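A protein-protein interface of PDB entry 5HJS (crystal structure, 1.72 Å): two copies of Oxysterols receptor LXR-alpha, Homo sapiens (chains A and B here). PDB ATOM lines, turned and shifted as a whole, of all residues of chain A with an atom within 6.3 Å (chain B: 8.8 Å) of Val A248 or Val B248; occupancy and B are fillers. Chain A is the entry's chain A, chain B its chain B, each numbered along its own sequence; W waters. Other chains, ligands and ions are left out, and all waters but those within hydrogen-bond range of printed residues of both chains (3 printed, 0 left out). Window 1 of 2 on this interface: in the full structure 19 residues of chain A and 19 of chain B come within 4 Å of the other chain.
The guanidinium group of Arg A251 lies within hydrogen-bond range of the side-chain hydroxyl of Thr B252 (2.7 Å). The side-chain carboxylate (OD2) of Asp B204 is in hydrogen-bond range of the side-chain hydroxyl (OG) of Ser A249 (2.9 Å). The side-chain hydroxyl (OG1) of Thr A252 lies within hydrogen-bond range of the guanidinium group (NH1) of Arg B251 (3.1 Å). The side-chain carboxylate of Asp A204 lies within hydrogen-bond range of the side-chain hydroxyl of Ser B249, 2.9 Å away.
The side-chain hydroxyl (OG) of Ser B202 lies within hydrogen-bond range of the backbone carbonyl oxygen (O) of Ile B198, at 3.4 Å. The guanidinium group of Arg B251 is in salt-bridge range of the side-chain carboxylate of Glu B132. The backbone carbonyl oxygen (O) of Ile B198 is in hydrogen-bond range of the side-chain amide nitrogen (NE2) of Gln B218 (3.0 Å). The guanidinium group (NH2) of Arg A251 is in salt-bridge range of the side-chain carboxylate (OD1) of Asp A204. The side-chain carboxylate of Glu A132 is in salt-bridge range of the guanidinium group of Arg A251. The side-chain carboxylate of Asp B204 is in salt-bridge range of the guanidinium group of Arg B251, 2.8 Å away.
CD1 of Leu A244 touches CB of Pro B241, at 3.5 Å. CG2 of Ile B198 touches CE of Met A245, at 3.6 Å. Gln B218 touches Met A245 (NE2 to CE, 3.2 Å). CD1 of Leu B247 touches CE of Met A245, at 3.8 Å. Leu A247 touches Met B245. Val B248 touches Leu A247 (CG1 to O, 3.7 Å). CG2 of Val A248 touches CG2 of Val B248, 3.7 Å away. CG1 of Val A248 touches CG of Arg B251, 3.5 Å away. Val B248 touches Arg A251. Arg A251 touches Arg B251.
Printed residues of chain B within 4 Å of Val A248: Leu B247, Val B248 and Arg B251. Val B248 touches three residues of chain A. Printed residues of chain B within 4 Å of Ser A249: Asp B204. Of the printed residues of chain A, Ile B198 touches Met A245 (3.6 Å). Printed residues of chain A within 4 Å of Met B245: Leu A247. Of the printed residues of chain B, Leu A244 touches Pro B241 (3.5 Å). Of the printed residues of chain A, Ser B249 touches Asp A204. The nearest residue of chain A that does not touch Val B248 is Leu A244 (4.8 Å). The nearest printed residue of chain B that does not touch Arg A251 is Ser B249 (4.3 Å).
Of the 24 printed residues of chain B, 10 touch a printed residue of chain A. Along chain A the printed residues that touch a printed residue of chain B span positions 204 to 252. Among the printed residues, 15 pairs touch across the chains. Among the printed residues, no Asp or Glu carboxylate lies within 4 Å of a Lys or Arg side-chain nitrogen of the other chain.
Asp A204 touches Ser B249, and with the chains exchanged Ser A249 touches Asp B204. Leu A247 touches Val B248, and with the chains exchanged Val A248 touches Leu B247. Arg A251 touches its own counterpart, Arg B251. Arg A251 touches Thr B252, and with the chains exchanged Thr A252 touches Arg B251. Positions printed for both chains: 132, 202, 204, 244, 245, 246, 247, 248, 249, 250, 251, 252 and 253. Of the 15 pairs that touch across the chains among the printed residues, 12 have their exchanged pair printed and touching as well.
Water W1 lies within hydrogen-bond range of the backbone carbonyl oxygen of Arg A251 (2.7 Å) and the side-chain hydroxyl of Thr B252 (3.2 Å). Water W3 bridges OD2 of Asp A204 (3.1 Å) and O of Ser B249 (3.3 Å). Water W2 bridges OD2 of Asp B204 (3.3 Å) and O of Ser A249 (3.3 Å).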
ATOM      1  N   GLU A 132      31.774 -13.180  -4.250  1.00  0.00           N
ATOM      2  CA  GLU A 132      30.674 -12.599  -3.480  1.00  0.00           C
ATOM      3  C   GLU A 132      29.737 -11.891  -4.430  1.00  0.00           C
ATOM      4  O   GLU A 132      28.533 -12.085  -4.346  1.00  0.00           O
ATOM      5  CB  GLU A 132      31.201 -11.663  -2.377  1.00  0.00           C
ATOM      6  CG  GLU A 132      32.108 -12.357  -1.385  1.00  0.00           C
ATOM      7  CD  GLU A 132      32.560 -11.516  -0.205  1.00  0.00           C
ATOM      8  OE1 GLU A 132      32.008 -10.411   0.000  1.00  0.00           O
ATOM      9  OE2 GLU A 132      33.468 -11.971   0.522  1.00  0.00           O
ATOM     10  N   SER A 202      35.714  -3.368   0.324  1.00  0.00           N
ATOM     11  CA  SER A 202      35.948  -3.828   1.699  1.00  0.00           C
ATOM     12  C   SER A 202      37.438  -3.658   2.041  1.00  0.00           C
ATOM     13  O   SER A 202      38.274  -4.360   1.466  1.00  0.00           O
ATOM     14  CB  SER A 202      35.544  -5.289   1.864  1.00  0.00           C
ATOM     15  OG  SER A 202      34.264  -5.534   1.316  1.00  0.00           O
ATOM     16  N   ASP A 204      39.116  -4.661   4.504  1.00  0.00           N
ATOM     17  CA  ASP A 204      39.641  -5.843   5.200  1.00  0.00           C
ATOM     18  C   ASP A 204      40.079  -6.994   4.263  1.00  0.00           C
ATOM     19  O   ASP A 204      40.541  -8.026   4.757  1.00  0.00           O
ATOM     20  CB  ASP A 204      38.628  -6.331   6.247  1.00  0.00           C
ATOM     21  CG  ASP A 204      37.369  -6.982   5.689  1.00  0.00           C
ATOM     22  OD1 ASP A 204      37.011  -6.689   4.528  1.00  0.00           O
ATOM     23  OD2 ASP A 204      36.736  -7.767   6.418  1.00  0.00           O
ATOM     24  N   LEU A 244      22.493  -4.986   4.622  1.00  0.00           N
ATOM     25  CA  LEU A 244      23.893  -4.998   5.041  1.00  0.00           C
ATOM     26  C   LEU A 244      24.289  -6.331   5.634  1.00  0.00           C
ATOM     27  O   LEU A 244      25.393  -6.772   5.374  1.00  0.00           O
ATOM     28  CB  LEU A 244      24.206  -3.898   6.064  1.00  0.00           C
ATOM     29  CG  LEU A 244      24.316  -2.478   5.563  1.00  0.00           C
ATOM     30  CD1 LEU A 244      24.833  -1.590   6.685  1.00  0.00           C
ATOM     31  CD2 LEU A 244      25.200  -2.372   4.271  1.00  0.00           C
ATOM     32  N   MET A 245      23.408  -6.966   6.435  1.00  0.00           N
ATOM     33  CA  MET A 245      23.676  -8.249   7.097  1.00  0.00           C
ATOM     34  C   MET A 245      23.864  -9.411   6.103  1.00  0.00           C
ATOM     35  O   MET A 245      24.435 -10.440   6.452  1.00  0.00           O
ATOM     36  CB  MET A 245      22.604  -8.578   8.159  1.00  0.00           C
ATOM     37  CG  MET A 245      22.553  -7.557   9.314  1.00  0.00           C
ATOM     38  SD  MET A 245      23.983  -7.608  10.400  1.00  0.00           S
ATOM     39  CE  MET A 245      23.598  -9.041  11.323  1.00  0.00           C
ATOM     40  N   LYS A 246      23.425  -9.232   4.856  1.00  0.00           N
ATOM     41  CA  LYS A 246      23.575 -10.254   3.820  1.00  0.00           C
ATOM     42  C   LYS A 246      25.040 -10.374   3.406  1.00  0.00           C
ATOM     43  O   LYS A 246      25.438 -11.421   2.926  1.00  0.00           O
ATOM     44  CB  LYS A 246      22.670  -9.947   2.616  1.00  0.00           C
ATOM     45  CG  LYS A 246      21.221 -10.287   2.897  1.00  0.00           C
ATOM     46  CD  LYS A 246      20.999 -11.809   2.955  1.00  0.00           C
ATOM     47  CE  LYS A 246      19.588 -12.170   3.331  1.00  0.00           C
ATOM     48  NZ  LYS A 246      19.486 -12.499   4.769  1.00  0.00           N
ATOM     49  N   LEU A 247      25.834  -9.300   3.615  1.00  0.00           N
ATOM     50  CA  LEU A 247      27.266  -9.256   3.321  1.00  0.00           C
ATOM     51  C   LEU A 247      28.002 -10.162   4.307  1.00  0.00           C
ATOM     52  O   LEU A 247      29.110 -10.634   4.009  1.00  0.00           O
ATOM     53  CB  LEU A 247      27.774  -7.815   3.450  1.00  0.00           C
ATOM     54  CG  LEU A 247      27.765  -6.864   2.220  1.00  0.00           C
ATOM     55  CD1 LEU A 247      26.811  -7.289   1.122  1.00  0.00           C
ATOM     56  CD2 LEU A 247      27.478  -5.470   2.637  1.00  0.00           C
ATOM     57  N   VAL A 248      27.398 -10.380   5.495  1.00  0.00           N
ATOM     58  CA  VAL A 248      27.937 -11.239   6.555  1.00  0.00           C
ATOM     59  C   VAL A 248      27.851 -12.689   6.018  1.00  0.00           C
ATOM     60  O   VAL A 248      28.840 -13.407   6.048  1.00  0.00           O
ATOM     61  CB  VAL A 248      27.168 -11.038   7.884  1.00  0.00           C
ATOM     62  CG1 VAL A 248      27.755 -11.905   8.987  1.00  0.00           C
ATOM     63  CG2 VAL A 248      27.136  -9.573   8.295  1.00  0.00           C
ATOM     64  N   SER A 249      26.684 -13.083   5.482  1.00  0.00           N
ATOM     65  CA  SER A 249      26.448 -14.418   4.889  1.00  0.00           C
ATOM     66  C   SER A 249      27.332 -14.673   3.668  1.00  0.00           C
ATOM     67  O   SER A 249      27.779 -15.806   3.479  1.00  0.00           O
ATOM     68  CB  SER A 249      24.981 -14.564   4.502  1.00  0.00           C
ATOM     69  OG  SER A 249      24.192 -14.313   5.648  1.00  0.00           O
ATOM     70  N   LEU A 250      27.605 -13.628   2.848  1.00  0.00           N
ATOM     71  CA  LEU A 250      28.492 -13.745   1.677  1.00  0.00           C
ATOM     72  C   LEU A 250      29.916 -14.110   2.057  1.00  0.00           C
ATOM     73  O   LEU A 250      30.567 -14.806   1.279  1.00  0.00           O
ATOM     74  CB  LEU A 250      28.526 -12.477   0.825  1.00  0.00           C
ATOM     75  CG  LEU A 250      27.372 -12.235  -0.107  1.00  0.00           C
ATOM     76  CD1 LEU A 250      27.380 -10.791  -0.560  1.00  0.00           C
ATOM     77  CD2 LEU A 250      27.431 -13.168  -1.338  1.00  0.00           C
ATOM     78  N   ARG A 251      30.416 -13.655   3.235  1.00  0.00           N
ATOM     79  CA  ARG A 251      31.774 -14.009   3.683  1.00  0.00           C
ATOM     80  C   ARG A 251      31.903 -15.484   3.914  1.00  0.00           C
ATOM     81  O   ARG A 251      32.950 -16.038   3.610  1.00  0.00           O
ATOM     82  CB  ARG A 251      32.187 -13.302   4.988  1.00  0.00           C
ATOM     83  CG  ARG A 251      32.689 -11.938   4.795  1.00  0.00           C
ATOM     84  CD  ARG A 251      33.756 -11.806   3.725  1.00  0.00           C
ATOM     85  NE  ARG A 251      33.914 -10.388   3.419  1.00  0.00           N
ATOM     86  CZ  ARG A 251      34.766  -9.611   4.051  1.00  0.00           C
ATOM     87  NH1 ARG A 251      35.556 -10.111   4.985  1.00  0.00           N
ATOM     88  NH2 ARG A 251      34.846  -8.330   3.751  1.00  0.00           N
ATOM     89  N   THR A 252      30.858 -16.116   4.491  1.00  0.00           N
ATOM     90  CA  THR A 252      30.835 -17.552   4.745  1.00  0.00           C
ATOM     91  C   THR A 252      30.773 -18.292   3.432  1.00  0.00           C
ATOM     92  O   THR A 252      31.500 -19.269   3.265  1.00  0.00           O
ATOM     93  CB  THR A 252      29.706 -17.939   5.713  1.00  0.00           C
ATOM     94  OG1 THR A 252      29.934 -17.252   6.933  1.00  0.00           O
ATOM     95  CG2 THR A 252      29.662 -19.447   5.987  1.00  0.00           C
ATOM     96  N   LEU A 253      29.935 -17.816   2.493  1.00  0.00           N
ATOM     97  CA  LEU A 253      29.794 -18.434   1.183  1.00  0.00           C
ATOM     98  C   LEU A 253      31.120 -18.437   0.448  1.00  0.00           C
ATOM     99  O   LEU A 253      31.443 -19.408  -0.218  1.00  0.00           O
ATOM    100  CB  LEU A 253      28.739 -17.708   0.350  1.00  0.00           C
ATOM    101  CG  LEU A 253      27.378 -18.392   0.244  1.00  0.00           C
ATOM    102  CD1 LEU A 253      26.471 -17.596  -0.636  1.00  0.00           C
ATOM    103  CD2 LEU A 253      27.484 -19.789  -0.358  1.00  0.00           C
ATOM    104  N   GLU B 132      33.767 -15.833  17.244  1.00  0.00           N
ATOM    105  CA  GLU B 132      33.498 -14.433  16.895  1.00  0.00           C
ATOM    106  C   GLU B 132      33.355 -13.613  18.160  1.00  0.00           C
ATOM    107  O   GLU B 132      33.914 -12.525  18.238  1.00  0.00           O
ATOM    108  CB  GLU B 132      32.214 -14.336  16.062  1.00  0.00           C
ATOM    109  CG  GLU B 132      32.335 -15.033  14.729  1.00  0.00           C
ATOM    110  CD  GLU B 132      31.112 -14.904  13.850  1.00  0.00           C
ATOM    111  OE1 GLU B 132      30.271 -14.007  14.098  1.00  0.00           O
ATOM    112  OE2 GLU B 132      30.996 -15.710  12.903  1.00  0.00           O
ATOM    113  N   PHE B 178      42.208  -6.885  13.245  1.00  0.00           N
ATOM    114  CA  PHE B 178      40.796  -6.702  13.631  1.00  0.00           C
ATOM    115  C   PHE B 178      40.693  -5.879  14.915  1.00  0.00           C
ATOM    116  O   PHE B 178      39.842  -4.993  15.016  1.00  0.00           O
ATOM    117  CB  PHE B 178      40.101  -8.059  13.847  1.00  0.00           C
ATOM    118  CG  PHE B 178      38.664  -7.928  14.292  1.00  0.00           C
ATOM    119  CD1 PHE B 178      37.671  -7.547  13.393  1.00  0.00           C
ATOM    120  CD2 PHE B 178      38.304  -8.162  15.618  1.00  0.00           C
ATOM    121  CE1 PHE B 178      36.339  -7.421  13.813  1.00  0.00           C
ATOM    122  CE2 PHE B 178      36.975  -8.054  16.030  1.00  0.00           C
ATOM    123  CZ  PHE B 178      36.006  -7.669  15.130  1.00  0.00           C
ATOM    124  N   LEU B 195      26.456  -5.974  19.981  1.00  0.00           N
ATOM    125  CA  LEU B 195      27.071  -6.644  18.826  1.00  0.00           C
ATOM    126  C   LEU B 195      27.260  -8.131  19.102  1.00  0.00           C
ATOM    127  O   LEU B 195      27.168  -8.973  18.187  1.00  0.00           O
ATOM    128  CB  LEU B 195      28.418  -6.021  18.496  1.00  0.00           C
ATOM    129  CG  LEU B 195      28.424  -4.894  17.476  1.00  0.00           C
ATOM    130  CD1 LEU B 195      29.875  -4.462  17.189  1.00  0.00           C
ATOM    131  CD2 LEU B 195      27.759  -5.298  16.156  1.00  0.00           C
ATOM    132  N   ILE B 198      23.877  -9.717  18.608  1.00  0.00           N
ATOM    133  CA  ILE B 198      23.596  -9.841  17.166  1.00  0.00           C
ATOM    134  C   ILE B 198      24.393 -11.016  16.549  1.00  0.00           C
ATOM    135  O   ILE B 198      23.872 -11.766  15.710  1.00  0.00           O
ATOM    136  CB  ILE B 198      23.848  -8.478  16.441  1.00  0.00           C
ATOM    137  CG1 ILE B 198      22.883  -7.429  17.015  1.00  0.00           C
ATOM    138  CG2 ILE B 198      23.686  -8.591  14.909  1.00  0.00           C
ATOM    139  CD1 ILE B 198      23.306  -5.914  16.780  1.00  0.00           C
ATOM    140  N   SER B 199      25.633 -11.175  16.986  1.00  0.00           N
ATOM    141  CA  SER B 199      26.514 -12.239  16.529  1.00  0.00           C
ATOM    142  C   SER B 199      25.945 -13.597  16.949  1.00  0.00           C
ATOM    143  O   SER B 199      25.962 -14.539  16.148  1.00  0.00           O
ATOM    144  CB  SER B 199      27.929 -12.048  17.081  1.00  0.00           C
ATOM    145  OG  SER B 199      28.735 -13.154  16.696  1.00  0.00           O
ATOM    146  N   SER B 202      22.453 -15.343  14.830  1.00  0.00           N
ATOM    147  CA  SER B 202      22.579 -15.341  13.378  1.00  0.00           C
ATOM    148  C   SER B 202      21.878 -16.582  12.833  1.00  0.00           C
ATOM    149  O   SER B 202      22.355 -17.695  13.037  1.00  0.00           O
ATOM    150  CB  SER B 202      24.047 -15.291  12.950  1.00  0.00           C
ATOM    151  OG  SER B 202      24.742 -14.300  13.687  1.00  0.00           O
ATOM    152  N   ASP B 204      21.649 -17.785   9.905  1.00  0.00           N
ATOM    153  CA  ASP B 204      22.375 -18.471   8.839  1.00  0.00           C
ATOM    154  C   ASP B 204      23.442 -19.435   9.352  1.00  0.00           C
ATOM    155  O   ASP B 204      24.180 -19.999   8.536  1.00  0.00           O
ATOM    156  CB  ASP B 204      22.954 -17.436   7.867  1.00  0.00           C
ATOM    157  CG  ASP B 204      24.068 -16.571   8.442  1.00  0.00           C
ATOM    158  OD1 ASP B 204      24.002 -16.231   9.644  1.00  0.00           O
ATOM    159  OD2 ASP B 204      24.999 -16.228   7.689  1.00  0.00           O
ATOM    160  N   ARG B 205      23.542 -19.635  10.693  1.00  0.00           N
ATOM    161  CA  ARG B 205      24.543 -20.566  11.249  1.00  0.00           C
ATOM    162  C   ARG B 205      24.191 -21.974  10.838  1.00  0.00           C
ATOM    163  O   ARG B 205      23.000 -22.278  10.749  1.00  0.00           O
ATOM    164  CB  ARG B 205      24.607 -20.576  12.800  1.00  0.00           C
ATOM    165  CG  ARG B 205      25.087 -19.313  13.501  1.00  0.00           C
ATOM    166  CD  ARG B 205      26.350 -18.683  12.982  1.00  0.00           C
ATOM    167  NE  ARG B 205      26.786 -17.625  13.897  1.00  0.00           N
ATOM    168  CZ  ARG B 205      27.827 -16.834  13.692  1.00  0.00           C
ATOM    169  NH1 ARG B 205      28.562 -16.966  12.600  1.00  0.00           N
ATOM    170  NH2 ARG B 205      28.121 -15.881  14.561  1.00  0.00           N
ATOM    171  N   GLN B 218      17.309 -11.444  16.380  1.00  0.00           N
ATOM    172  CA  GLN B 218      18.427 -10.617  15.926  1.00  0.00           C
ATOM    173  C   GLN B 218      17.987  -9.181  15.653  1.00  0.00           C
ATOM    174  O   GLN B 218      18.633  -8.225  16.105  1.00  0.00           O
ATOM    175  CB  GLN B 218      19.060 -11.195  14.651  1.00  0.00           C
ATOM    176  CG  GLN B 218      20.471 -10.663  14.452  1.00  0.00           C
ATOM    177  CD  GLN B 218      21.098 -11.010  13.138  1.00  0.00           C
ATOM    178  OE1 GLN B 218      20.482 -10.915  12.084  1.00  0.00           O
ATOM    179  NE2 GLN B 218      22.356 -11.403  13.174  1.00  0.00           N
ATOM    180  N   PRO B 241      25.958   1.524  10.833  1.00  0.00           N
ATOM    181  CA  PRO B 241      26.375   0.497   9.853  1.00  0.00           C
ATOM    182  C   PRO B 241      27.836   0.075  10.017  1.00  0.00           C
ATOM    183  O   PRO B 241      28.123  -1.097   9.794  1.00  0.00           O
ATOM    184  CB  PRO B 241      26.089   1.150   8.497  1.00  0.00           C
ATOM    185  CG  PRO B 241      26.076   2.613   8.775  1.00  0.00           C
ATOM    186  CD  PRO B 241      25.510   2.756  10.145  1.00  0.00           C
ATOM    187  N   ARG B 242      28.758   0.981  10.471  1.00  0.00           N
ATOM    188  CA  ARG B 242      30.169   0.624  10.698  1.00  0.00           C
ATOM    189  C   ARG B 242      30.299  -0.505  11.727  1.00  0.00           C
ATOM    190  O   ARG B 242      31.107  -1.414  11.534  1.00  0.00           O
ATOM    191  CB  ARG B 242      31.024   1.844  11.145  1.00  0.00           C
ATOM    192  CG  ARG B 242      31.346   2.809  10.019  1.00  0.00           C
ATOM    193  CD  ARG B 242      32.123   4.009  10.504  1.00  0.00           C
ATOM    194  NE  ARG B 242      33.507   3.651  10.843  1.00  0.00           N
ATOM    195  CZ  ARG B 242      34.374   4.465  11.432  1.00  0.00           C
ATOM    196  NH1 ARG B 242      34.018   5.697  11.758  1.00  0.00           N
ATOM    197  NH2 ARG B 242      35.605   4.051  11.705  1.00  0.00           N
ATOM    198  N   MET B 243      29.492  -0.473  12.803  1.00  0.00           N
ATOM    199  CA  MET B 243      29.528  -1.528  13.812  1.00  0.00           C
ATOM    200  C   MET B 243      28.992  -2.816  13.235  1.00  0.00           C
ATOM    201  O   MET B 243      29.557  -3.865  13.505  1.00  0.00           O
ATOM    202  CB  MET B 243      28.699  -1.167  15.073  1.00  0.00           C
ATOM    203  CG  MET B 243      29.213   0.006  15.823  1.00  0.00           C
ATOM    204  SD  MET B 243      28.067   0.478  17.142  1.00  0.00           S
ATOM    205  CE  MET B 243      28.672   2.192  17.449  1.00  0.00           C
ATOM    206  N   LEU B 244      27.887  -2.756  12.460  1.00  0.00           N
ATOM    207  CA  LEU B 244      27.342  -3.967  11.852  1.00  0.00           C
ATOM    208  C   LEU B 244      28.324  -4.576  10.898  1.00  0.00           C
ATOM    209  O   LEU B 244      28.443  -5.788  10.869  1.00  0.00           O
ATOM    210  CB  LEU B 244      26.035  -3.716  11.092  1.00  0.00           C
ATOM    211  CG  LEU B 244      24.807  -3.281  11.875  1.00  0.00           C
ATOM    212  CD1 LEU B 244      23.671  -3.075  10.918  1.00  0.00           C
ATOM    213  CD2 LEU B 244      24.404  -4.331  12.900  1.00  0.00           C
ATOM    214  N   MET B 245      29.035  -3.740  10.115  1.00  0.00           N
ATOM    215  CA  MET B 245      30.018  -4.187   9.126  1.00  0.00           C
ATOM    216  C   MET B 245      31.177  -4.933   9.775  1.00  0.00           C
ATOM    217  O   MET B 245      31.861  -5.688   9.094  1.00  0.00           O
ATOM    218  CB  MET B 245      30.510  -3.038   8.241  1.00  0.00           C
ATOM    219  CG  MET B 245      29.421  -2.456   7.276  1.00  0.00           C
ATOM    220  SD  MET B 245      28.682  -3.646   6.119  1.00  0.00           S
ATOM    221  CE  MET B 245      30.006  -3.778   4.917  1.00  0.00           C
ATOM    222  N   LYS B 246      31.377  -4.762  11.100  1.00  0.00           N
ATOM    223  CA  LYS B 246      32.443  -5.480  11.776  1.00  0.00           C
ATOM    224  C   LYS B 246      32.086  -6.951  11.874  1.00  0.00           C
ATOM    225  O   LYS B 246      32.984  -7.767  11.939  1.00  0.00           O
ATOM    226  CB  LYS B 246      32.833  -4.840  13.120  1.00  0.00           C
ATOM    227  CG  LYS B 246      33.594  -3.519  12.920  1.00  0.00           C
ATOM    228  CD  LYS B 246      35.088  -3.772  12.657  1.00  0.00           C
ATOM    229  CE  LYS B 246      35.864  -2.544  12.259  1.00  0.00           C
ATOM    230  NZ  LYS B 246      35.742  -2.269  10.813  1.00  0.00           N
ATOM    231  N   LEU B 247      30.776  -7.289  11.784  1.00  0.00           N
ATOM    232  CA  LEU B 247      30.288  -8.686  11.801  1.00  0.00           C
ATOM    233  C   LEU B 247      30.650  -9.444  10.531  1.00  0.00           C
ATOM    234  O   LEU B 247      30.658 -10.672  10.556  1.00  0.00           O
ATOM    235  CB  LEU B 247      28.766  -8.780  12.029  1.00  0.00           C
ATOM    236  CG  LEU B 247      28.215  -8.260  13.380  1.00  0.00           C
ATOM    237  CD1 LEU B 247      26.753  -8.259  13.353  1.00  0.00           C
ATOM    238  CD2 LEU B 247      28.690  -9.112  14.547  1.00  0.00           C
ATOM    239  N   VAL B 248      30.935  -8.715   9.429  1.00  0.00           N
ATOM    240  CA  VAL B 248      31.329  -9.259   8.136  1.00  0.00           C
ATOM    241  C   VAL B 248      32.766  -9.786   8.348  1.00  0.00           C
ATOM    242  O   VAL B 248      33.038 -10.952   8.073  1.00  0.00           O
ATOM    243  CB  VAL B 248      31.301  -8.158   7.035  1.00  0.00           C
ATOM    244  CG1 VAL B 248      31.782  -8.721   5.701  1.00  0.00           C
ATOM    245  CG2 VAL B 248      29.906  -7.539   6.872  1.00  0.00           C
ATOM    246  N   SER B 249      33.661  -8.915   8.867  1.00  0.00           N
ATOM    247  CA  SER B 249      35.079  -9.191   9.172  1.00  0.00           C
ATOM    248  C   SER B 249      35.209 -10.382  10.119  1.00  0.00           C
ATOM    249  O   SER B 249      36.110 -11.197   9.926  1.00  0.00           O
ATOM    250  CB  SER B 249      35.737  -7.966   9.806  1.00  0.00           C
ATOM    251  OG  SER B 249      35.607  -6.848   8.944  1.00  0.00           O
ATOM    252  N   LEU B 250      34.309 -10.483  11.123  1.00  0.00           N
ATOM    253  CA  LEU B 250      34.279 -11.575  12.096  1.00  0.00           C
ATOM    254  C   LEU B 250      34.061 -12.913  11.427  1.00  0.00           C
ATOM    255  O   LEU B 250      34.644 -13.903  11.860  1.00  0.00           O
ATOM    256  CB  LEU B 250      33.223 -11.359  13.198  1.00  0.00           C
ATOM    257  CG  LEU B 250      33.622 -10.503  14.367  1.00  0.00           C
ATOM    258  CD1 LEU B 250      32.424 -10.200  15.201  1.00  0.00           C
ATOM    259  CD2 LEU B 250      34.740 -11.162  15.196  1.00  0.00           C
ATOM    260  N   ARG B 251      33.237 -12.969  10.364  1.00  0.00           N
ATOM    261  CA  ARG B 251      33.016 -14.222   9.638  1.00  0.00           C
ATOM    262  C   ARG B 251      34.273 -14.686   8.955  1.00  0.00           C
ATOM    263  O   ARG B 251      34.463 -15.879   8.859  1.00  0.00           O
ATOM    264  CB  ARG B 251      31.927 -14.116   8.578  1.00  0.00           C
ATOM    265  CG  ARG B 251      30.560 -14.064   9.120  1.00  0.00           C
ATOM    266  CD  ARG B 251      30.104 -15.341   9.796  1.00  0.00           C
ATOM    267  NE  ARG B 251      28.784 -15.089  10.366  1.00  0.00           N
ATOM    268  CZ  ARG B 251      27.637 -15.491   9.843  1.00  0.00           C
ATOM    269  NH1 ARG B 251      27.622 -16.226   8.737  1.00  0.00           N
ATOM    270  NH2 ARG B 251      26.492 -15.200  10.446  1.00  0.00           N
ATOM    271  N   THR B 252      35.092 -13.770   8.420  1.00  0.00           N
ATOM    272  CA  THR B 252      36.369 -14.132   7.776  1.00  0.00           C
ATOM    273  C   THR B 252      37.340 -14.664   8.830  1.00  0.00           C
ATOM    274  O   THR B 252      38.000 -15.668   8.600  1.00  0.00           O
ATOM    275  CB  THR B 252      36.963 -12.951   7.014  1.00  0.00           C
ATOM    276  OG1 THR B 252      36.075 -12.620   5.957  1.00  0.00           O
ATOM    277  CG2 THR B 252      38.355 -13.252   6.463  1.00  0.00           C
ATOM    278  N   LEU B 253      37.389 -14.025   9.993  1.00  0.00           N
ATOM    279  CA  LEU B 253      38.246 -14.441  11.101  1.00  0.00           C
ATOM    280  C   LEU B 253      37.888 -15.828  11.621  1.00  0.00           C
ATOM    281  O   LEU B 253      38.769 -16.605  11.997  1.00  0.00           O
ATOM    282  CB  LEU B 253      38.145 -13.429  12.231  1.00  0.00           C
ATOM    283  CG  LEU B 253      39.046 -12.225  12.118  1.00  0.00           C
ATOM    284  CD1 LEU B 253      38.536 -11.125  12.994  1.00  0.00           C
ATOM    285  CD2 LEU B 253      40.458 -12.575  12.539  1.00  0.00           C
ATOM    286  N   SER B 254      36.596 -16.150  11.607  1.00  0.00           N
ATOM    287  CA  SER B 254      36.115 -17.452  12.020  1.00  0.00           C
ATOM    288  C   SER B 254      36.650 -18.522  11.065  1.00  0.00           C
ATOM    289  O   SER B 254      36.955 -19.623  11.500  1.00  0.00           O
ATOM    290  CB  SER B 254      34.593 -17.466  12.059  1.00  0.00           C
ATOM    291  OG  SER B 254      34.160 -18.793  12.279  1.00  0.00           O
ATOM    292  N   SER B 255      36.744 -18.200   9.777  1.00  0.00           N
ATOM    293  CA  SER B 255      37.246 -19.088   8.731  1.00  0.00           C
ATOM    294  C   SER B 255      38.773 -19.254   8.876  1.00  0.00           C
ATOM    295  O   SER B 255      39.267 -20.351   8.725  1.00  0.00           O
ATOM    296  CB  SER B 255      36.891 -18.527   7.360  1.00  0.00           C
ATOM    297  OG  SER B 255      37.527 -19.265   6.329  1.00  0.00           O
HETATM  298  O   HOH W   1      35.499 -15.222   4.123  1.00  0.00           O
HETATM  299  O   HOH W   2      26.292 -18.076   5.334  1.00  0.00           O
HETATM  300  O   HOH W   3      38.325 -10.001   7.864  1.00  0.00           O
